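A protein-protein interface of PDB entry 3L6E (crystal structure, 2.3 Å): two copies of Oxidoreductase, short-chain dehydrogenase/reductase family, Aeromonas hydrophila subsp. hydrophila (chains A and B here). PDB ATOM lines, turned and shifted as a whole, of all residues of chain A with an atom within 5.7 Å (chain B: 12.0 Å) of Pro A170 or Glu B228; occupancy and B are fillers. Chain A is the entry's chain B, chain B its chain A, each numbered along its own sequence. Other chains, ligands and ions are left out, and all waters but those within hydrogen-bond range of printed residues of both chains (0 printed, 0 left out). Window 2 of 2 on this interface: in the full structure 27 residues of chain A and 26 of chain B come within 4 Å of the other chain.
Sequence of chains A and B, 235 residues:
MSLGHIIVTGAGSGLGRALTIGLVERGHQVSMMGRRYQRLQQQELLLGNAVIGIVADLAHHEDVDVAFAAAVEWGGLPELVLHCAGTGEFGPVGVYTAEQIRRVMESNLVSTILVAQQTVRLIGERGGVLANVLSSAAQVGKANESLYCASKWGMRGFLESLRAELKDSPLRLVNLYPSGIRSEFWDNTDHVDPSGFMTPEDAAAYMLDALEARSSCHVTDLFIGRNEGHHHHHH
N of Gly B225 lies within hydrogen-bond range of O of His A218 (2.8 Å). A ring nitrogen (ND1) of His A218 lies within hydrogen-bond range of the side-chain amide oxygen (OD1) of Asn B227 (2.8 Å).
The backbone carbonyl oxygen of Ile B224 sits at hydrogen-bond distance from the backbone NH of Ser B179. O of Leu A166 lies within hydrogen-bond range of OG of Ser A169. O of Gly A128 sits at hydrogen-bond distance from N of Arg A172, 2.9 Å away.
Among the printed residues, pairs that only touch across the chains: His A218 with Arg B226 (3.3 Å), Arg A172 with Asn B227 (3.5 Å), His A218 with Ile B224 (3.5 Å), His A218 with Tyr B206 (3.6 Å), Ser A169 with Glu B228 (3.8 Å), Pro A170 with Glu B228 (3.8 Å) and Arg A172 with Glu B228 (3.9 Å).
Pro A170 touches just one residue of chain B: Glu B228. Glu B228 touches three residues of chain A. No residue of chain B comes within 4 Å of Gly A127. No residue of chain B comes within 4 Å of Gly A128. No residue of chain B comes within 4 Å of Leu A171. Of chain B, only Asn B227 (3.5 Å) and Glu B228 (3.9 Å) come within 4 Å of Arg A172. Of the printed residues of chain A, Arg B226 touches His A218 (3.3 Å). Of the printed residues of chain A, Gly B225 touches His A218. Of the printed residues of chain A, Tyr B206 touches His A218. Met B198 touches none of the printed residues of chain A. Thr B199 touches none of the printed residues of chain A.
Printed residues of chain B that touch a printed residue of chain A: Tyr B206, Ile B224, Gly B225, Arg B226, Asn B227 and Glu B228. Hydrophobic or aromatic side chains of chain B that line the printed part of chain A: Tyr B206 and Ile B224.
No position is printed for both chains. Of the 9 pairs that touch across the chains among the printed residues, none has its exchanged pair printed and touching as well.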
ATOM      1  N   ILE A 123     -31.487 -25.840  19.246  1.00  0.00           N
ATOM      2  CA  ILE A 123     -31.153 -25.870  20.669  1.00  0.00           C
ATOM      3  C   ILE A 123     -30.671 -24.535  21.230  1.00  0.00           C
ATOM      4  O   ILE A 123     -30.109 -24.497  22.328  1.00  0.00           O
ATOM      5  CB  ILE A 123     -30.118 -27.009  20.999  1.00  0.00           C
ATOM      6  CG1 ILE A 123     -28.738 -26.703  20.413  1.00  0.00           C
ATOM      7  CG2 ILE A 123     -30.645 -28.353  20.529  1.00  0.00           C
ATOM      8  CD1 ILE A 123     -27.604 -27.607  20.993  1.00  0.00           C
ATOM      9  N   GLY A 124     -30.891 -23.456  20.481  1.00  0.00           N
ATOM     10  CA  GLY A 124     -30.434 -22.128  20.886  1.00  0.00           C
ATOM     11  C   GLY A 124     -31.046 -21.618  22.174  1.00  0.00           C
ATOM     12  O   GLY A 124     -30.350 -20.999  22.985  1.00  0.00           O
ATOM     13  N   GLU A 125     -32.342 -21.884  22.368  1.00  0.00           N
ATOM     14  CA  GLU A 125     -33.080 -21.418  23.544  1.00  0.00           C
ATOM     15  C   GLU A 125     -32.924 -22.395  24.695  1.00  0.00           C
ATOM     16  O   GLU A 125     -32.796 -22.006  25.850  1.00  0.00           O
ATOM     17  CB  GLU A 125     -34.578 -21.272  23.225  1.00  0.00           C
ATOM     18  CG  GLU A 125     -35.045 -19.852  22.955  1.00  0.00           C
ATOM     19  CD  GLU A 125     -34.871 -19.439  21.505  1.00  0.00           C
ATOM     20  OE1 GLU A 125     -35.902 -19.318  20.802  1.00  0.00           O
ATOM     21  OE2 GLU A 125     -33.711 -19.244  21.069  1.00  0.00           O
ATOM     22  N   ARG A 126     -32.968 -23.673  24.351  1.00  0.00           N
ATOM     23  CA  ARG A 126     -32.844 -24.754  25.304  1.00  0.00           C
ATOM     24  C   ARG A 126     -31.436 -24.762  25.901  1.00  0.00           C
ATOM     25  O   ARG A 126     -31.262 -24.887  27.125  1.00  0.00           O
ATOM     26  CB  ARG A 126     -33.174 -26.072  24.598  1.00  0.00           C
ATOM     27  CG  ARG A 126     -32.804 -27.304  25.363  1.00  0.00           C
ATOM     28  CD  ARG A 126     -33.027 -28.569  24.565  1.00  0.00           C
ATOM     29  NE  ARG A 126     -32.175 -29.612  25.125  1.00  0.00           N
ATOM     30  CZ  ARG A 126     -32.482 -30.363  26.179  1.00  0.00           C
ATOM     31  NH1 ARG A 126     -33.664 -30.238  26.791  1.00  0.00           N
ATOM     32  NH2 ARG A 126     -31.599 -31.259  26.612  1.00  0.00           N
ATOM     33  N   GLY A 127     -30.436 -24.592  25.043  1.00  0.00           N
ATOM     34  CA  GLY A 127     -29.056 -24.607  25.487  1.00  0.00           C
ATOM     35  C   GLY A 127     -28.430 -25.951  25.187  1.00  0.00           C
ATOM     36  O   GLY A 127     -29.123 -26.870  24.755  1.00  0.00           O
ATOM     37  N   GLY A 128     -27.132 -26.073  25.472  1.00  0.00           N
ATOM     38  CA  GLY A 128     -26.312 -27.181  24.990  1.00  0.00           C
ATOM     39  C   GLY A 128     -24.995 -26.666  24.410  1.00  0.00           C
ATOM     40  O   GLY A 128     -24.595 -25.534  24.672  1.00  0.00           O
ATOM     41  N   LEU A 166     -23.731 -14.621  20.507  1.00  0.00           N
ATOM     42  CA  LEU A 166     -24.570 -15.490  21.336  1.00  0.00           C
ATOM     43  C   LEU A 166     -24.335 -15.336  22.834  1.00  0.00           C
ATOM     44  O   LEU A 166     -24.907 -16.082  23.629  1.00  0.00           O
ATOM     45  CB  LEU A 166     -24.384 -16.963  20.941  1.00  0.00           C
ATOM     46  CG  LEU A 166     -24.905 -17.464  19.591  1.00  0.00           C
ATOM     47  CD1 LEU A 166     -24.487 -18.907  19.402  1.00  0.00           C
ATOM     48  CD2 LEU A 166     -26.419 -17.329  19.439  1.00  0.00           C
ATOM     49  N   LYS A 167     -23.505 -14.373  23.218  1.00  0.00           N
ATOM     50  CA  LYS A 167     -23.163 -14.127  24.628  1.00  0.00           C
ATOM     51  C   LYS A 167     -24.289 -14.338  25.655  1.00  0.00           C
ATOM     52  O   LYS A 167     -24.062 -14.907  26.725  1.00  0.00           O
ATOM     53  CB  LYS A 167     -22.573 -12.721  24.807  1.00  0.00           C
ATOM     54  CG  LYS A 167     -21.226 -12.742  25.532  1.00  0.00           C
ATOM     55  CD  LYS A 167     -20.991 -11.509  26.405  1.00  0.00           C
ATOM     56  CE  LYS A 167     -20.049 -11.849  27.565  1.00  0.00           C
ATOM     57  NZ  LYS A 167     -20.624 -12.912  28.460  1.00  0.00           N
ATOM     58  N   ASP A 168     -25.493 -13.871  25.339  1.00  0.00           N
ATOM     59  CA  ASP A 168     -26.577 -13.891  26.314  1.00  0.00           C
ATOM     60  C   ASP A 168     -27.565 -15.015  26.045  1.00  0.00           C
ATOM     61  O   ASP A 168     -28.785 -14.851  26.197  1.00  0.00           O
ATOM     62  CB  ASP A 168     -27.255 -12.521  26.365  1.00  0.00           C
ATOM     63  CG  ASP A 168     -26.320 -11.439  26.870  1.00  0.00           C
ATOM     64  OD1 ASP A 168     -26.440 -10.282  26.415  1.00  0.00           O
ATOM     65  OD2 ASP A 168     -25.449 -11.758  27.713  1.00  0.00           O
ATOM     66  N   SER A 169     -27.013 -16.170  25.666  1.00  0.00           N
ATOM     67  CA  SER A 169     -27.810 -17.321  25.313  1.00  0.00           C
ATOM     68  C   SER A 169     -27.184 -18.596  25.879  1.00  0.00           C
ATOM     69  O   SER A 169     -25.964 -18.677  26.071  1.00  0.00           O
ATOM     70  CB  SER A 169     -27.990 -17.403  23.797  1.00  0.00           C
ATOM     71  OG  SER A 169     -26.815 -17.906  23.174  1.00  0.00           O
ATOM     72  N   PRO A 170     -28.023 -19.597  26.172  1.00  0.00           N
ATOM     73  CA  PRO A 170     -27.527 -20.814  26.820  1.00  0.00           C
ATOM     74  C   PRO A 170     -26.784 -21.776  25.878  1.00  0.00           C
ATOM     75  O   PRO A 170     -26.157 -22.733  26.342  1.00  0.00           O
ATOM     76  CB  PRO A 170     -28.807 -21.451  27.359  1.00  0.00           C
ATOM     77  CG  PRO A 170     -29.852 -21.008  26.389  1.00  0.00           C
ATOM     78  CD  PRO A 170     -29.493 -19.591  26.064  1.00  0.00           C
ATOM     79  N   LEU A 171     -26.855 -21.545  24.576  1.00  0.00           N
ATOM     80  CA  LEU A 171     -26.046 -22.324  23.635  1.00  0.00           C
ATOM     81  C   LEU A 171     -24.573 -21.890  23.689  1.00  0.00           C
ATOM     82  O   LEU A 171     -24.243 -20.724  23.439  1.00  0.00           O
ATOM     83  CB  LEU A 171     -26.603 -22.266  22.205  1.00  0.00           C
ATOM     84  CG  LEU A 171     -25.786 -22.939  21.079  1.00  0.00           C
ATOM     85  CD1 LEU A 171     -25.517 -24.443  21.281  1.00  0.00           C
ATOM     86  CD2 LEU A 171     -26.406 -22.715  19.722  1.00  0.00           C
ATOM     87  N   ARG A 172     -23.694 -22.836  24.025  1.00  0.00           N
ATOM     88  CA  ARG A 172     -22.280 -22.511  24.215  1.00  0.00           C
ATOM     89  C   ARG A 172     -21.495 -22.984  23.007  1.00  0.00           C
ATOM     90  O   ARG A 172     -21.744 -24.065  22.469  1.00  0.00           O
ATOM     91  CB  ARG A 172     -21.718 -23.139  25.509  1.00  0.00           C
ATOM     92  CG  ARG A 172     -22.578 -22.914  26.753  1.00  0.00           C
ATOM     93  CD  ARG A 172     -21.801 -23.099  28.049  1.00  0.00           C
ATOM     94  NE  ARG A 172     -21.976 -24.410  28.678  1.00  0.00           N
ATOM     95  CZ  ARG A 172     -22.647 -24.624  29.817  1.00  0.00           C
ATOM     96  NH1 ARG A 172     -22.730 -25.852  30.318  1.00  0.00           N
ATOM     97  NH2 ARG A 172     -23.242 -23.620  30.464  1.00  0.00           N
ATOM     98  N   HIS A 218     -16.877 -24.189  31.818  1.00  0.00           N
ATOM     99  CA  HIS A 218     -16.666 -25.092  30.695  1.00  0.00           C
ATOM    100  C   HIS A 218     -15.469 -24.615  29.860  1.00  0.00           C
ATOM    101  O   HIS A 218     -15.145 -23.416  29.839  1.00  0.00           O
ATOM    102  CB  HIS A 218     -17.920 -25.161  29.809  1.00  0.00           C
ATOM    103  CG  HIS A 218     -18.204 -23.882  29.088  1.00  0.00           C
ATOM    104  ND1 HIS A 218     -18.711 -22.767  29.726  1.00  0.00           N
ATOM    105  CD2 HIS A 218     -18.018 -23.523  27.793  1.00  0.00           C
ATOM    106  CE1 HIS A 218     -18.823 -21.779  28.857  1.00  0.00           C
ATOM    107  NE2 HIS A 218     -18.417 -22.212  27.676  1.00  0.00           N
ATOM    108  N   SER B 179     -10.822 -18.201  32.996  1.00  0.00           N
ATOM    109  CA  SER B 179     -11.422 -16.866  33.086  1.00  0.00           C
ATOM    110  C   SER B 179     -12.679 -16.886  33.929  1.00  0.00           C
ATOM    111  O   SER B 179     -13.688 -17.483  33.538  1.00  0.00           O
ATOM    112  CB  SER B 179     -11.784 -16.331  31.704  1.00  0.00           C
ATOM    113  OG  SER B 179     -10.667 -15.736  31.084  1.00  0.00           O
ATOM    114  N   GLY B 180     -12.621 -16.225  35.082  1.00  0.00           N
ATOM    115  CA  GLY B 180     -13.812 -16.043  35.912  1.00  0.00           C
ATOM    116  C   GLY B 180     -13.708 -16.704  37.268  1.00  0.00           C
ATOM    117  O   GLY B 180     -14.708 -17.181  37.813  1.00  0.00           O
ATOM    118  N   PHE B 197     -17.596 -16.841  39.533  1.00  0.00           N
ATOM    119  CA  PHE B 197     -18.465 -17.979  39.823  1.00  0.00           C
ATOM    120  C   PHE B 197     -17.813 -19.336  39.461  1.00  0.00           C
ATOM    121  O   PHE B 197     -18.333 -20.379  39.838  1.00  0.00           O
ATOM    122  CB  PHE B 197     -19.822 -17.815  39.125  1.00  0.00           C
ATOM    123  CG  PHE B 197     -21.008 -18.225  39.973  1.00  0.00           C
ATOM    124  CD1 PHE B 197     -22.052 -17.326  40.210  1.00  0.00           C
ATOM    125  CD2 PHE B 197     -21.090 -19.505  40.530  1.00  0.00           C
ATOM    126  CE1 PHE B 197     -23.150 -17.695  40.990  1.00  0.00           C
ATOM    127  CE2 PHE B 197     -22.179 -19.882  41.311  1.00  0.00           C
ATOM    128  CZ  PHE B 197     -23.214 -18.975  41.544  1.00  0.00           C
ATOM    129  N   MET B 198     -16.688 -19.322  38.744  1.00  0.00           N
ATOM    130  CA  MET B 198     -15.912 -20.550  38.487  1.00  0.00           C
ATOM    131  C   MET B 198     -15.251 -21.048  39.775  1.00  0.00           C
ATOM    132  O   MET B 198     -14.530 -20.311  40.433  1.00  0.00           O
ATOM    133  CB  MET B 198     -14.845 -20.312  37.410  1.00  0.00           C
ATOM    134  CG  MET B 198     -13.900 -21.504  37.132  1.00  0.00           C
ATOM    135  SD  MET B 198     -12.492 -21.103  35.811  1.00  0.00           S
ATOM    136  CE  MET B 198     -13.607 -20.383  34.391  1.00  0.00           C
ATOM    137  N   THR B 199     -15.510 -22.297  40.147  1.00  0.00           N
ATOM    138  CA  THR B 199     -14.872 -22.853  41.347  1.00  0.00           C
ATOM    139  C   THR B 199     -13.465 -23.336  41.012  1.00  0.00           C
ATOM    140  O   THR B 199     -13.229 -23.791  39.906  1.00  0.00           O
ATOM    141  CB  THR B 199     -15.677 -24.022  41.975  1.00  0.00           C
ATOM    142  OG1 THR B 199     -15.558 -25.196  41.172  1.00  0.00           O
ATOM    143  CG2 THR B 199     -17.136 -23.662  42.140  1.00  0.00           C
ATOM    144  N   ASP B 202     -13.476 -27.300  39.857  1.00  0.00           N
ATOM    145  CA  ASP B 202     -13.836 -27.521  38.461  1.00  0.00           C
ATOM    146  C   ASP B 202     -12.723 -27.031  37.512  1.00  0.00           C
ATOM    147  O   ASP B 202     -12.370 -27.721  36.535  1.00  0.00           O
ATOM    148  CB  ASP B 202     -15.131 -26.791  38.121  1.00  0.00           C
ATOM    149  CG  ASP B 202     -16.378 -27.402  38.766  1.00  0.00           C
ATOM    150  OD1 ASP B 202     -16.384 -28.564  39.252  1.00  0.00           O
ATOM    151  OD2 ASP B 202     -17.396 -26.685  38.739  1.00  0.00           O
ATOM    152  N   TYR B 206     -10.459 -29.683  34.845  1.00  0.00           N
ATOM    153  CA  TYR B 206     -10.186 -29.482  33.418  1.00  0.00           C
ATOM    154  C   TYR B 206      -8.698 -29.405  33.126  1.00  0.00           C
ATOM    155  O   TYR B 206      -8.231 -30.003  32.169  1.00  0.00           O
ATOM    156  CB  TYR B 206     -10.814 -28.188  32.885  1.00  0.00           C
ATOM    157  CG  TYR B 206     -12.288 -28.290  32.600  1.00  0.00           C
ATOM    158  CD1 TYR B 206     -12.789 -29.282  31.752  1.00  0.00           C
ATOM    159  CD2 TYR B 206     -13.182 -27.407  33.187  1.00  0.00           C
ATOM    160  CE1 TYR B 206     -14.156 -29.376  31.503  1.00  0.00           C
ATOM    161  CE2 TYR B 206     -14.523 -27.488  32.933  1.00  0.00           C
ATOM    162  CZ  TYR B 206     -15.003 -28.460  32.090  1.00  0.00           C
ATOM    163  OH  TYR B 206     -16.360 -28.517  31.865  1.00  0.00           O
ATOM    164  N   ILE B 224     -10.663 -21.792  29.724  1.00  0.00           N
ATOM    165  CA  ILE B 224     -11.886 -22.144  30.457  1.00  0.00           C
ATOM    166  C   ILE B 224     -12.680 -20.884  30.755  1.00  0.00           C
ATOM    167  O   ILE B 224     -12.119 -19.913  31.250  1.00  0.00           O
ATOM    168  CB  ILE B 224     -11.571 -22.838  31.798  1.00  0.00           C
ATOM    169  CG1 ILE B 224     -10.597 -24.005  31.596  1.00  0.00           C
ATOM    170  CG2 ILE B 224     -12.858 -23.335  32.475  1.00  0.00           C
ATOM    171  CD1 ILE B 224      -9.871 -24.353  32.872  1.00  0.00           C
ATOM    172  N   GLY B 225     -13.986 -20.907  30.478  1.00  0.00           N
ATOM    173  CA  GLY B 225     -14.866 -19.763  30.773  1.00  0.00           C
ATOM    174  C   GLY B 225     -16.010 -20.124  31.702  1.00  0.00           C
ATOM    175  O   GLY B 225     -16.382 -21.291  31.806  1.00  0.00           O
ATOM    176  N   ARG B 226     -16.567 -19.108  32.373  1.00  0.00           N
ATOM    177  CA  ARG B 226     -17.744 -19.271  33.235  1.00  0.00           C
ATOM    178  C   ARG B 226     -18.966 -19.794  32.488  1.00  0.00           C
ATOM    179  O   ARG B 226     -19.134 -19.543  31.299  1.00  0.00           O
ATOM    180  CB  ARG B 226     -18.122 -17.952  33.909  1.00  0.00           C
ATOM    181  CG  ARG B 226     -17.194 -17.506  35.035  1.00  0.00           C
ATOM    182  CD  ARG B 226     -17.906 -16.561  36.033  1.00  0.00           C
ATOM    183  NE  ARG B 226     -18.739 -15.548  35.382  1.00  0.00           N
ATOM    184  CZ  ARG B 226     -18.297 -14.391  34.885  1.00  0.00           C
ATOM    185  NH1 ARG B 226     -17.005 -14.072  34.949  1.00  0.00           N
ATOM    186  NH2 ARG B 226     -19.155 -13.546  34.310  1.00  0.00           N
ATOM    187  N   ASN B 227     -19.814 -20.530  33.200  1.00  0.00           N
ATOM    188  CA  ASN B 227     -21.091 -20.952  32.651  1.00  0.00           C
ATOM    189  C   ASN B 227     -22.128 -19.823  32.677  1.00  0.00           C
ATOM    190  O   ASN B 227     -22.030 -18.890  33.480  1.00  0.00           O
ATOM    191  CB  ASN B 227     -21.614 -22.189  33.391  1.00  0.00           C
ATOM    192  CG  ASN B 227     -20.880 -23.454  32.999  1.00  0.00           C
ATOM    193  OD1 ASN B 227     -20.086 -23.453  32.058  1.00  0.00           O
ATOM    194  ND2 ASN B 227     -21.150 -24.546  33.706  1.00  0.00           N
ATOM    195  N   GLU B 228     -23.108 -19.913  31.785  1.00  0.00           N
ATOM    196  CA  GLU B 228     -24.220 -18.961  31.736  1.00  0.00           C
ATOM    197  C   GLU B 228     -25.143 -19.193  32.934  1.00  0.00           C
ATOM    198  O   GLU B 228     -25.236 -20.315  33.441  1.00  0.00           O
ATOM    199  CB  GLU B 228     -24.995 -19.130  30.423  1.00  0.00           C
ATOM    200  CG  GLU B 228     -25.380 -17.829  29.747  1.00  0.00           C
ATOM    201  CD  GLU B 228     -26.771 -17.360  30.117  1.00  0.00           C
ATOM    202  OE1 GLU B 228     -27.748 -17.878  29.533  1.00  0.00           O
ATOM    203  OE2 GLU B 228     -26.890 -16.456  30.976  1.00  0.00           O
ATOM    204  N   GLY B 229     -25.818 -18.130  33.377  1.00  0.00           N
ATOM    205  CA  GLY B 229     -26.709 -18.190  34.540  1.00  0.00           C
ATOM    206  C   GLY B 229     -27.970 -18.996  34.293  1.00  0.00           C
ATOM    207  O   GLY B 229     -28.551 -18.948  33.208  1.00  0.00           O
